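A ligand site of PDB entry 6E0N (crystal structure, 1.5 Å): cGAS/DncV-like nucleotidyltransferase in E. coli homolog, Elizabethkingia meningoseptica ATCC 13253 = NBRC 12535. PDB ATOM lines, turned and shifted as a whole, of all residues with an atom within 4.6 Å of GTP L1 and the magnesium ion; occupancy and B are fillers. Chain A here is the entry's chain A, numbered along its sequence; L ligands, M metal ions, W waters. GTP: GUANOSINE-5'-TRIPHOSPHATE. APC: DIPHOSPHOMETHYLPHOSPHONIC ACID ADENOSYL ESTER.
The magnesium ion is bound by water W9 (2.0 Å). The magnesium ion is bound by O1A of GTP L1. The magnesium ion is bound by O1B of GTP L1. Water W11 binds the magnesium ion, at 2.1 Å. OD2 of Asp 63 is bound to the magnesium ion (2.2 Å). The magnesium ion is bound by an oxygen (O3G) of GTP L1, at 2.2 Å. The magnesium ion has six donor atoms within binding distance.
Residues that only touch GTP L1: Ile 168 (3.8 Å), Ser 169 (3.9 Å), Tyr 201 (3.6 Å), Phe 217 (3.3 Å) and Glu 220 (3.6 Å). Along chain A the residues within 4 Å of GTP L1 span positions 47 to 220.
The side-chain amide nitrogen (ND2) of Asn 52 lies within hydrogen-bond range of an oxygen (O3') of GTP L1, 3.2 Å away. The side-chain hydroxyl (OG) of Ser 216 sits close to an oxygen (O3B) of GTP L1 (3.1 Å). The backbone NH of Gly 48 sits close to an oxygen (O3') of GTP L1 (3.1 Å). The backbone NH (N) of Ser 49 sits at hydrogen-bond distance from an oxygen (O2B) of GTP L1 (3.0 Å). An oxygen (O4') of GTP L1 is in hydrogen-bond range of the side-chain amide nitrogen of Gln 47, 3.1 Å away. O3' of APC L2 lies within hydrogen-bond range of OD1 of Asp 63, at 2.8 Å. A nitrogen (N3) of APC L2 sits at hydrogen-bond distance from the side-chain amide nitrogen (NE2) of Gln 47, 2.8 Å away. The side-chain amino group of Lys 197 is in salt-bridge range of an oxygen (O1G) of GTP L1, at 3.1 Å.
NZ of Lys 197 sits at hydrogen-bond distance from OG of Ser 216 (3.0 Å). O of Asp 63 is in hydrogen-bond range of N of Gln 47 (3.2 Å). OG of Ser 216 sits at hydrogen-bond distance from OE2 of Glu 220 (2.9 Å). The side-chain amide nitrogen (ND2) of Asn 52 sits at hydrogen-bond distance from the backbone carbonyl oxygen (O) of Gly 48. The side-chain amino group of Lys 197 lies within hydrogen-bond range of the backbone carbonyl oxygen of Thr 54, at 2.8 Å. NE2 of His 174 is in hydrogen-bond range of OE1 of Glu 220 (2.7 Å). O of Ser 49 is in hydrogen-bond range of N of Thr 54 (2.9 Å). The side-chain amide nitrogen of Asn 55 sits close to the side-chain hydroxyl of Ser 49 (3.2 Å).
Water W11 lies within hydrogen-bond range of the side-chain hydroxyl of Ser 49 and the backbone carbonyl oxygen of Asp 61. Water W9 lies within hydrogen-bond range of the side-chain carboxylate of Asp 63 (2.5 Å) and an oxygen (O3') of APC L2 (3.4 Å). Water W6 bridges an oxygen (O2') of GTP L1 and the side-chain hydroxyl (OG) of Ser 169. Water W1 lies within hydrogen-bond range of O3' of GTP L1 (2.7 Å) and OE2 of Glu 220 (3.0 Å). Water W2 lies within hydrogen-bond range of OE2 of Glu 259 and N2 of GTP L1. Water W3 lies within hydrogen-bond range of a nitrogen (N6) of APC L2 (2.4 Å), the backbone carbonyl oxygen of Ile 168 (2.5 Å) and a nitrogen (N1) of GTP L1 (3.2 Å).
Within 4 Å of the magnesium ion: Asp 63. The nearest printed residue that does not touch the magnesium ion is Ser 49 (4.2 Å).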
ATOM      1  N   GLN A  47     -24.036   5.718   1.547  1.00  0.00           N
ATOM      2  CA  GLN A  47     -24.530   4.888   2.626  1.00  0.00           C
ATOM      3  C   GLN A  47     -25.432   5.762   3.491  1.00  0.00           C
ATOM      4  O   GLN A  47     -25.670   6.920   3.203  1.00  0.00           O
ATOM      5  CB  GLN A  47     -23.380   4.279   3.431  1.00  0.00           C
ATOM      6  CG  GLN A  47     -22.622   5.286   4.231  1.00  0.00           C
ATOM      7  CD  GLN A  47     -21.610   4.629   5.153  1.00  0.00           C
ATOM      8  OE1 GLN A  47     -21.312   3.449   5.003  1.00  0.00           O
ATOM      9  NE2 GLN A  47     -21.085   5.393   6.102  1.00  0.00           N
ATOM     10  N   GLY A  48     -25.931   5.192   4.561  1.00  0.00           N
ATOM     11  CA  GLY A  48     -26.734   5.947   5.501  1.00  0.00           C
ATOM     12  C   GLY A  48     -28.118   6.253   4.965  1.00  0.00           C
ATOM     13  O   GLY A  48     -28.618   5.623   4.022  1.00  0.00           O
ATOM     14  N   SER A  49     -28.735   7.270   5.570  1.00  0.00           N
ATOM     15  CA  SER A  49     -30.179   7.478   5.423  1.00  0.00           C
ATOM     16  C   SER A  49     -30.566   7.740   3.967  1.00  0.00           C
ATOM     17  O   SER A  49     -31.653   7.342   3.530  1.00  0.00           O
ATOM     18  CB  SER A  49     -30.622   8.643   6.309  1.00  0.00           C
ATOM     19  OG  SER A  49     -30.017   9.858   5.890  1.00  0.00           O
ATOM     20  N   ASN A  52     -30.442   4.186   2.267  1.00  0.00           N
ATOM     21  CA  ASN A  52     -31.480   3.300   2.749  1.00  0.00           C
ATOM     22  C   ASN A  52     -32.863   3.946   2.744  1.00  0.00           C
ATOM     23  O   ASN A  52     -33.851   3.269   3.039  1.00  0.00           O
ATOM     24  CB  ASN A  52     -31.124   2.813   4.151  1.00  0.00           C
ATOM     25  CG  ASN A  52     -29.719   2.227   4.220  1.00  0.00           C
ATOM     26  OD1 ASN A  52     -29.325   1.430   3.369  1.00  0.00           O
ATOM     27  ND2 ASN A  52     -28.955   2.640   5.223  1.00  0.00           N
ATOM     28  N   THR A  54     -34.194   6.455   4.706  1.00  0.00           N
ATOM     29  CA  THR A  54     -34.725   6.538   6.062  1.00  0.00           C
ATOM     30  C   THR A  54     -34.628   7.938   6.654  1.00  0.00           C
ATOM     31  O   THR A  54     -34.651   8.097   7.873  1.00  0.00           O
ATOM     32  CB  THR A  54     -34.006   5.537   6.966  1.00  0.00           C
ATOM     33  OG1 THR A  54     -32.599   5.829   6.990  1.00  0.00           O
ATOM     34  CG2 THR A  54     -34.217   4.105   6.481  1.00  0.00           C
ATOM     35  N   ASN A  55     -34.545   8.959   5.805  1.00  0.00           N
ATOM     36  CA  ASN A  55     -34.439  10.338   6.288  1.00  0.00           C
ATOM     37  C   ASN A  55     -35.786  10.838   6.798  1.00  0.00           C
ATOM     38  O   ASN A  55     -36.822  10.654   6.154  1.00  0.00           O
ATOM     39  CB  ASN A  55     -33.971  11.247   5.152  1.00  0.00           C
ATOM     40  CG  ASN A  55     -32.469  11.253   4.981  1.00  0.00           C
ATOM     41  OD1 ASN A  55     -31.731  11.407   5.950  1.00  0.00           O
ATOM     42  ND2 ASN A  55     -32.018  11.076   3.744  1.00  0.00           N
ATOM     43  N   ASP A  61     -27.986  15.677   6.236  1.00  0.00           N
ATOM     44  CA  ASP A  61     -26.652  15.450   5.688  1.00  0.00           C
ATOM     45  C   ASP A  61     -26.611  14.116   4.946  1.00  0.00           C
ATOM     46  O   ASP A  61     -27.270  13.147   5.334  1.00  0.00           O
ATOM     47  CB  ASP A  61     -25.617  15.412   6.811  1.00  0.00           C
ATOM     48  CG  ASP A  61     -25.600  16.680   7.651  1.00  0.00           C
ATOM     49  OD1 ASP A  61     -26.260  17.668   7.260  1.00  0.00           O
ATOM     50  OD2 ASP A  61     -24.928  16.682   8.704  1.00  0.00           O
ATOM     51  N   ASP A  63     -24.240  10.937   3.372  1.00  0.00           N
ATOM     52  CA  ASP A  63     -23.011  10.195   3.629  1.00  0.00           C
ATOM     53  C   ASP A  63     -22.483   9.653   2.303  1.00  0.00           C
ATOM     54  O   ASP A  63     -23.064   8.738   1.722  1.00  0.00           O
ATOM     55  CB  ASP A  63     -23.278   9.058   4.615  1.00  0.00           C
ATOM     56  CG  ASP A  63     -23.873   9.552   5.914  1.00  0.00           C
ATOM     57  OD1 ASP A  63     -23.316  10.515   6.482  1.00  0.00           O
ATOM     58  OD2 ASP A  63     -24.901   9.000   6.358  1.00  0.00           O
ATOM     59  N   ILE A 168     -15.676  -0.794  10.777  1.00  0.00           N
ATOM     60  CA  ILE A 168     -15.990  -1.767   9.736  1.00  0.00           C
ATOM     61  C   ILE A 168     -17.476  -1.712   9.440  1.00  0.00           C
ATOM     62  O   ILE A 168     -18.297  -1.621  10.370  1.00  0.00           O
ATOM     63  CB  ILE A 168     -15.536  -3.193  10.136  1.00  0.00           C
ATOM     64  CG1 ILE A 168     -14.005  -3.264  10.096  1.00  0.00           C
ATOM     65  CG2 ILE A 168     -16.187  -4.228   9.265  1.00  0.00           C
ATOM     66  CD1 ILE A 168     -13.422  -4.550  10.613  1.00  0.00           C
ATOM     67  N   SER A 169     -17.832  -1.762   8.166  1.00  0.00           N
ATOM     68  CA  SER A 169     -19.211  -1.591   7.730  1.00  0.00           C
ATOM     69  C   SER A 169     -19.458  -2.479   6.522  1.00  0.00           C
ATOM     70  O   SER A 169     -18.551  -2.759   5.739  1.00  0.00           O
ATOM     71  CB  SER A 169     -19.484  -0.122   7.379  1.00  0.00           C
ATOM     72  OG  SER A 169     -20.827   0.081   6.960  1.00  0.00           O
ATOM     73  N   HIS A 174     -26.327  -4.463   4.155  1.00  0.00           N
ATOM     74  CA  HIS A 174     -27.312  -3.701   4.905  1.00  0.00           C
ATOM     75  C   HIS A 174     -28.405  -3.167   3.987  1.00  0.00           C
ATOM     76  O   HIS A 174     -29.601  -3.337   4.254  1.00  0.00           O
ATOM     77  CB  HIS A 174     -26.594  -2.550   5.630  1.00  0.00           C
ATOM     78  CG  HIS A 174     -27.495  -1.739   6.518  1.00  0.00           C
ATOM     79  ND1 HIS A 174     -27.601  -1.976   7.868  1.00  0.00           N
ATOM     80  CD2 HIS A 174     -28.301  -0.696   6.242  1.00  0.00           C
ATOM     81  CE1 HIS A 174     -28.456  -1.104   8.395  1.00  0.00           C
ATOM     82  NE2 HIS A 174     -28.895  -0.323   7.428  1.00  0.00           N
ATOM     83  N   LYS A 197     -37.381   6.805  14.351  1.00  0.00           N
ATOM     84  CA  LYS A 197     -36.390   7.874  14.263  1.00  0.00           C
ATOM     85  C   LYS A 197     -37.005   9.224  14.619  1.00  0.00           C
ATOM     86  O   LYS A 197     -36.366  10.052  15.289  1.00  0.00           O
ATOM     87  CB  LYS A 197     -35.768   7.914  12.869  1.00  0.00           C
ATOM     88  CG  LYS A 197     -34.807   6.761  12.601  1.00  0.00           C
ATOM     89  CD  LYS A 197     -34.218   6.807  11.198  1.00  0.00           C
ATOM     90  CE  LYS A 197     -33.289   7.999  11.011  1.00  0.00           C
ATOM     91  NZ  LYS A 197     -32.541   7.919   9.724  1.00  0.00           N
ATOM     92  N   TYR A 201     -35.729  11.597  17.757  1.00  0.00           N
ATOM     93  CA  TYR A 201     -35.356  13.004  17.703  1.00  0.00           C
ATOM     94  C   TYR A 201     -36.182  13.833  18.680  1.00  0.00           C
ATOM     95  O   TYR A 201     -35.666  14.759  19.307  1.00  0.00           O
ATOM     96  CB  TYR A 201     -35.514  13.545  16.279  1.00  0.00           C
ATOM     97  CG  TYR A 201     -34.415  13.117  15.335  1.00  0.00           C
ATOM     98  CD1 TYR A 201     -33.078  13.310  15.655  1.00  0.00           C
ATOM     99  CD2 TYR A 201     -34.715  12.519  14.114  1.00  0.00           C
ATOM    100  CE1 TYR A 201     -32.071  12.916  14.797  1.00  0.00           C
ATOM    101  CE2 TYR A 201     -33.711  12.125  13.247  1.00  0.00           C
ATOM    102  CZ  TYR A 201     -32.394  12.325  13.595  1.00  0.00           C
ATOM    103  OH  TYR A 201     -31.379  11.936  12.734  1.00  0.00           O
ATOM    104  N   SER A 216     -29.466   5.677  14.244  1.00  0.00           N
ATOM    105  CA  SER A 216     -30.280   5.196  13.123  1.00  0.00           C
ATOM    106  C   SER A 216     -29.944   3.737  12.810  1.00  0.00           C
ATOM    107  O   SER A 216     -30.842   2.905  12.641  1.00  0.00           O
ATOM    108  CB  SER A 216     -30.050   6.082  11.894  1.00  0.00           C
ATOM    109  OG  SER A 216     -30.885   5.675  10.821  1.00  0.00           O
ATOM    110  N   PHE A 217     -28.646   3.423  12.727  1.00  0.00           N
ATOM    111  CA  PHE A 217     -28.237   2.044  12.480  1.00  0.00           C
ATOM    112  C   PHE A 217     -28.826   1.090  13.524  1.00  0.00           C
ATOM    113  O   PHE A 217     -29.362   0.039  13.176  1.00  0.00           O
ATOM    114  CB  PHE A 217     -26.708   1.963  12.484  1.00  0.00           C
ATOM    115  CG  PHE A 217     -26.172   0.576  12.318  1.00  0.00           C
ATOM    116  CD1 PHE A 217     -26.094   0.004  11.064  1.00  0.00           C
ATOM    117  CD2 PHE A 217     -25.763  -0.164  13.412  1.00  0.00           C
ATOM    118  CE1 PHE A 217     -25.611  -1.272  10.892  1.00  0.00           C
ATOM    119  CE2 PHE A 217     -25.271  -1.449  13.249  1.00  0.00           C
ATOM    120  CZ  PHE A 217     -25.199  -1.998  11.985  1.00  0.00           C
ATOM    121  N   GLU A 220     -32.517   0.626  12.986  1.00  0.00           N
ATOM    122  CA  GLU A 220     -32.748  -0.211  11.813  1.00  0.00           C
ATOM    123  C   GLU A 220     -32.518  -1.676  12.126  1.00  0.00           C
ATOM    124  O   GLU A 220     -33.277  -2.545  11.662  1.00  0.00           O
ATOM    125  CB  GLU A 220     -31.854   0.261  10.664  1.00  0.00           C
ATOM    126  CG  GLU A 220     -32.303   1.593  10.085  1.00  0.00           C
ATOM    127  CD  GLU A 220     -31.325   2.151   9.073  1.00  0.00           C
ATOM    128  OE1 GLU A 220     -30.823   1.383   8.224  1.00  0.00           O
ATOM    129  OE2 GLU A 220     -31.065   3.374   9.121  1.00  0.00           O
ATOM    130  N   GLU A 259     -27.337  -8.024  12.881  1.00  0.00           N
ATOM    131  CA  GLU A 259     -27.328  -6.800  12.104  1.00  0.00           C
ATOM    132  C   GLU A 259     -28.160  -7.017  10.852  1.00  0.00           C
ATOM    133  O   GLU A 259     -28.466  -8.158  10.476  1.00  0.00           O
ATOM    134  CB  GLU A 259     -25.893  -6.390  11.793  1.00  0.00           C
ATOM    135  CG  GLU A 259     -25.094  -6.078  13.064  1.00  0.00           C
ATOM    136  CD  GLU A 259     -23.659  -5.655  12.806  1.00  0.00           C
ATOM    137  OE1 GLU A 259     -23.121  -5.963  11.723  1.00  0.00           O
ATOM    138  OE2 GLU A 259     -23.074  -5.024  13.707  1.00  0.00           O
HETATM  139  PG  GTP L   1     -29.040   9.555  10.053  1.00  0.00           P
HETATM  140  O1G GTP L   1     -30.366  10.182   9.707  1.00  0.00           O
HETATM  141  O2G GTP L   1     -28.790   9.726  11.532  1.00  0.00           O
HETATM  142  O3G GTP L   1     -27.922  10.204   9.262  1.00  0.00           O
HETATM  143  O3B GTP L   1     -29.143   7.977   9.747  1.00  0.00           O
HETATM  144  PB  GTP L   1     -28.062   7.168   8.867  1.00  0.00           P
HETATM  145  O1B GTP L   1     -27.478   8.045   7.774  1.00  0.00           O
HETATM  146  O2B GTP L   1     -28.751   5.957   8.304  1.00  0.00           O
HETATM  147  O3A GTP L   1     -26.914   6.676   9.870  1.00  0.00           O
HETATM  148  PA  GTP L   1     -25.488   7.411  10.008  1.00  0.00           P
HETATM  149  O1A GTP L   1     -25.494   8.768   9.360  1.00  0.00           O
HETATM  150  O2A GTP L   1     -25.099   7.496  11.461  1.00  0.00           O
HETATM  151  O5' GTP L   1     -24.473   6.432   9.244  1.00  0.00           O
HETATM  152  C5' GTP L   1     -24.621   6.209   7.868  1.00  0.00           C
HETATM  153  C4' GTP L   1     -24.417   4.748   7.572  1.00  0.00           C
HETATM  154  O4' GTP L   1     -23.167   4.327   8.150  1.00  0.00           O
HETATM  155  C3' GTP L   1     -25.481   3.759   8.067  1.00  0.00           C
HETATM  156  O3' GTP L   1     -26.480   3.521   7.133  1.00  0.00           O
HETATM  157  C2' GTP L   1     -24.639   2.478   8.275  1.00  0.00           C
HETATM  158  O2' GTP L   1     -24.638   1.753   7.076  1.00  0.00           O
HETATM  159  C1' GTP L   1     -23.241   2.997   8.645  1.00  0.00           C
HETATM  160  N9  GTP L   1     -23.125   2.947  10.108  1.00  0.00           N
HETATM  161  C8  GTP L   1     -23.296   3.986  10.974  1.00  0.00           C
HETATM  162  N7  GTP L   1     -23.116   3.525  12.238  1.00  0.00           N
HETATM  163  C5  GTP L   1     -22.815   2.201  12.167  1.00  0.00           C
HETATM  164  C6  GTP L   1     -22.535   1.248  13.146  1.00  0.00           C
HETATM  165  O6  GTP L   1     -22.529   1.564  14.327  1.00  0.00           O
HETATM  166  N1  GTP L   1     -22.270  -0.053  12.768  1.00  0.00           N
HETATM  167  C2  GTP L   1     -22.284  -0.391  11.432  1.00  0.00           C
HETATM  168  N2  GTP L   1     -22.024  -1.648  11.054  1.00  0.00           N
HETATM  169  N3  GTP L   1     -22.563   0.548  10.464  1.00  0.00           N
HETATM  170  C4  GTP L   1     -22.821   1.831  10.829  1.00  0.00           C
HETATM  171  PG  APC L   2     -16.921  14.071  15.790  1.00  0.00           P
HETATM  172  O1G APC L   2     -18.258  14.728  15.565  1.00  0.00           O
HETATM  173  O2G APC L   2     -15.841  14.788  15.022  1.00  0.00           O
HETATM  174  O3G APC L   2     -16.595  14.089  17.259  1.00  0.00           O
HETATM  175  PB  APC L   2     -17.822  12.101  13.949  1.00  0.00           P
HETATM  176  O1B APC L   2     -18.787  13.144  13.529  1.00  0.00           O
HETATM  177  O2B APC L   2     -16.978  11.581  12.846  1.00  0.00           O
HETATM  178  O3B APC L   2     -16.988  12.507  15.278  1.00  0.00           O
HETATM  179  PA  APC L   2     -20.438  10.605  13.384  1.00  0.00           P
HETATM  180  O1A APC L   2     -21.009  11.971  13.169  1.00  0.00           O
HETATM  181  O2A APC L   2     -21.493   9.715  14.075  1.00  0.00           O
HETATM  182  C3A APC L   2     -18.908  10.763  14.455  1.00  0.00           C
HETATM  183  O5' APC L   2     -19.977   9.816  12.007  1.00  0.00           O
HETATM  184  C5' APC L   2     -19.547  10.635  10.973  1.00  0.00           C
HETATM  185  C4' APC L   2     -19.910   9.923   9.652  1.00  0.00           C
HETATM  186  O4' APC L   2     -19.175   8.864   9.529  1.00  0.00           O
HETATM  187  C3' APC L   2     -21.376   9.457   9.722  1.00  0.00           C
HETATM  188  O3' APC L   2     -22.168  10.322   9.042  1.00  0.00           O
HETATM  189  C2' APC L   2     -21.359   8.070   9.054  1.00  0.00           C
HETATM  190  O2' APC L   2     -21.787   8.206   7.629  1.00  0.00           O
HETATM  191  C1' APC L   2     -20.139   7.634   9.111  1.00  0.00           C
HETATM  192  N9  APC L   2     -20.042   6.606  10.140  1.00  0.00           N
HETATM  193  C8  APC L   2     -20.068   6.634  11.481  1.00  0.00           C
HETATM  194  N7  APC L   2     -19.940   5.378  11.931  1.00  0.00           N
HETATM  195  C5  APC L   2     -19.848   4.564  10.873  1.00  0.00           C
HETATM  196  C6  APC L   2     -19.707   3.199  10.746  1.00  0.00           C
HETATM  197  N6  APC L   2     -19.615   2.112  11.693  1.00  0.00           N
HETATM  198  N1  APC L   2     -19.643   2.643   9.549  1.00  0.00           N
HETATM  199  C2  APC L   2     -19.704   3.410   8.443  1.00  0.00           C
HETATM  200  N3  APC L   2     -19.829   4.750   8.565  1.00  0.00           N
HETATM  201  C4  APC L   2     -19.916   5.325   9.770  1.00  0.00           C
HETATM  202 MG    MG M   1     -26.313   9.832   7.797  1.00  0.00          MG
HETATM  203  O   HOH W   1     -28.080   3.208   9.230  1.00  0.00           O
HETATM  204  O   HOH W   2     -20.801  -3.725  13.126  1.00  0.00           O
HETATM  205  O   HOH W   3     -19.105  -0.164  12.297  1.00  0.00           O
HETATM  206  O   HOH W   4     -24.358   3.222  15.450  1.00  0.00           O
HETATM  207  O   HOH W   5     -33.198  11.473   9.498  1.00  0.00           O
HETATM  208  O   HOH W   6     -23.526  -0.411   7.230  1.00  0.00           O
HETATM  209  O   HOH W   7     -26.377   5.377  12.635  1.00  0.00           O
HETATM  210  O   HOH W   8     -23.218  -3.121   8.341  1.00  0.00           O
HETATM  211  O   HOH W   9     -25.153  11.468   7.967  1.00  0.00           O
HETATM  212  O   HOH W  10     -21.605  -1.533  14.959  1.00  0.00           O
HETATM  213  O   HOH W  11     -27.474  10.546   6.150  1.00  0.00           O
HETATM  214  O   HOH W  12     -24.541  10.922  10.397  1.00  0.00           O
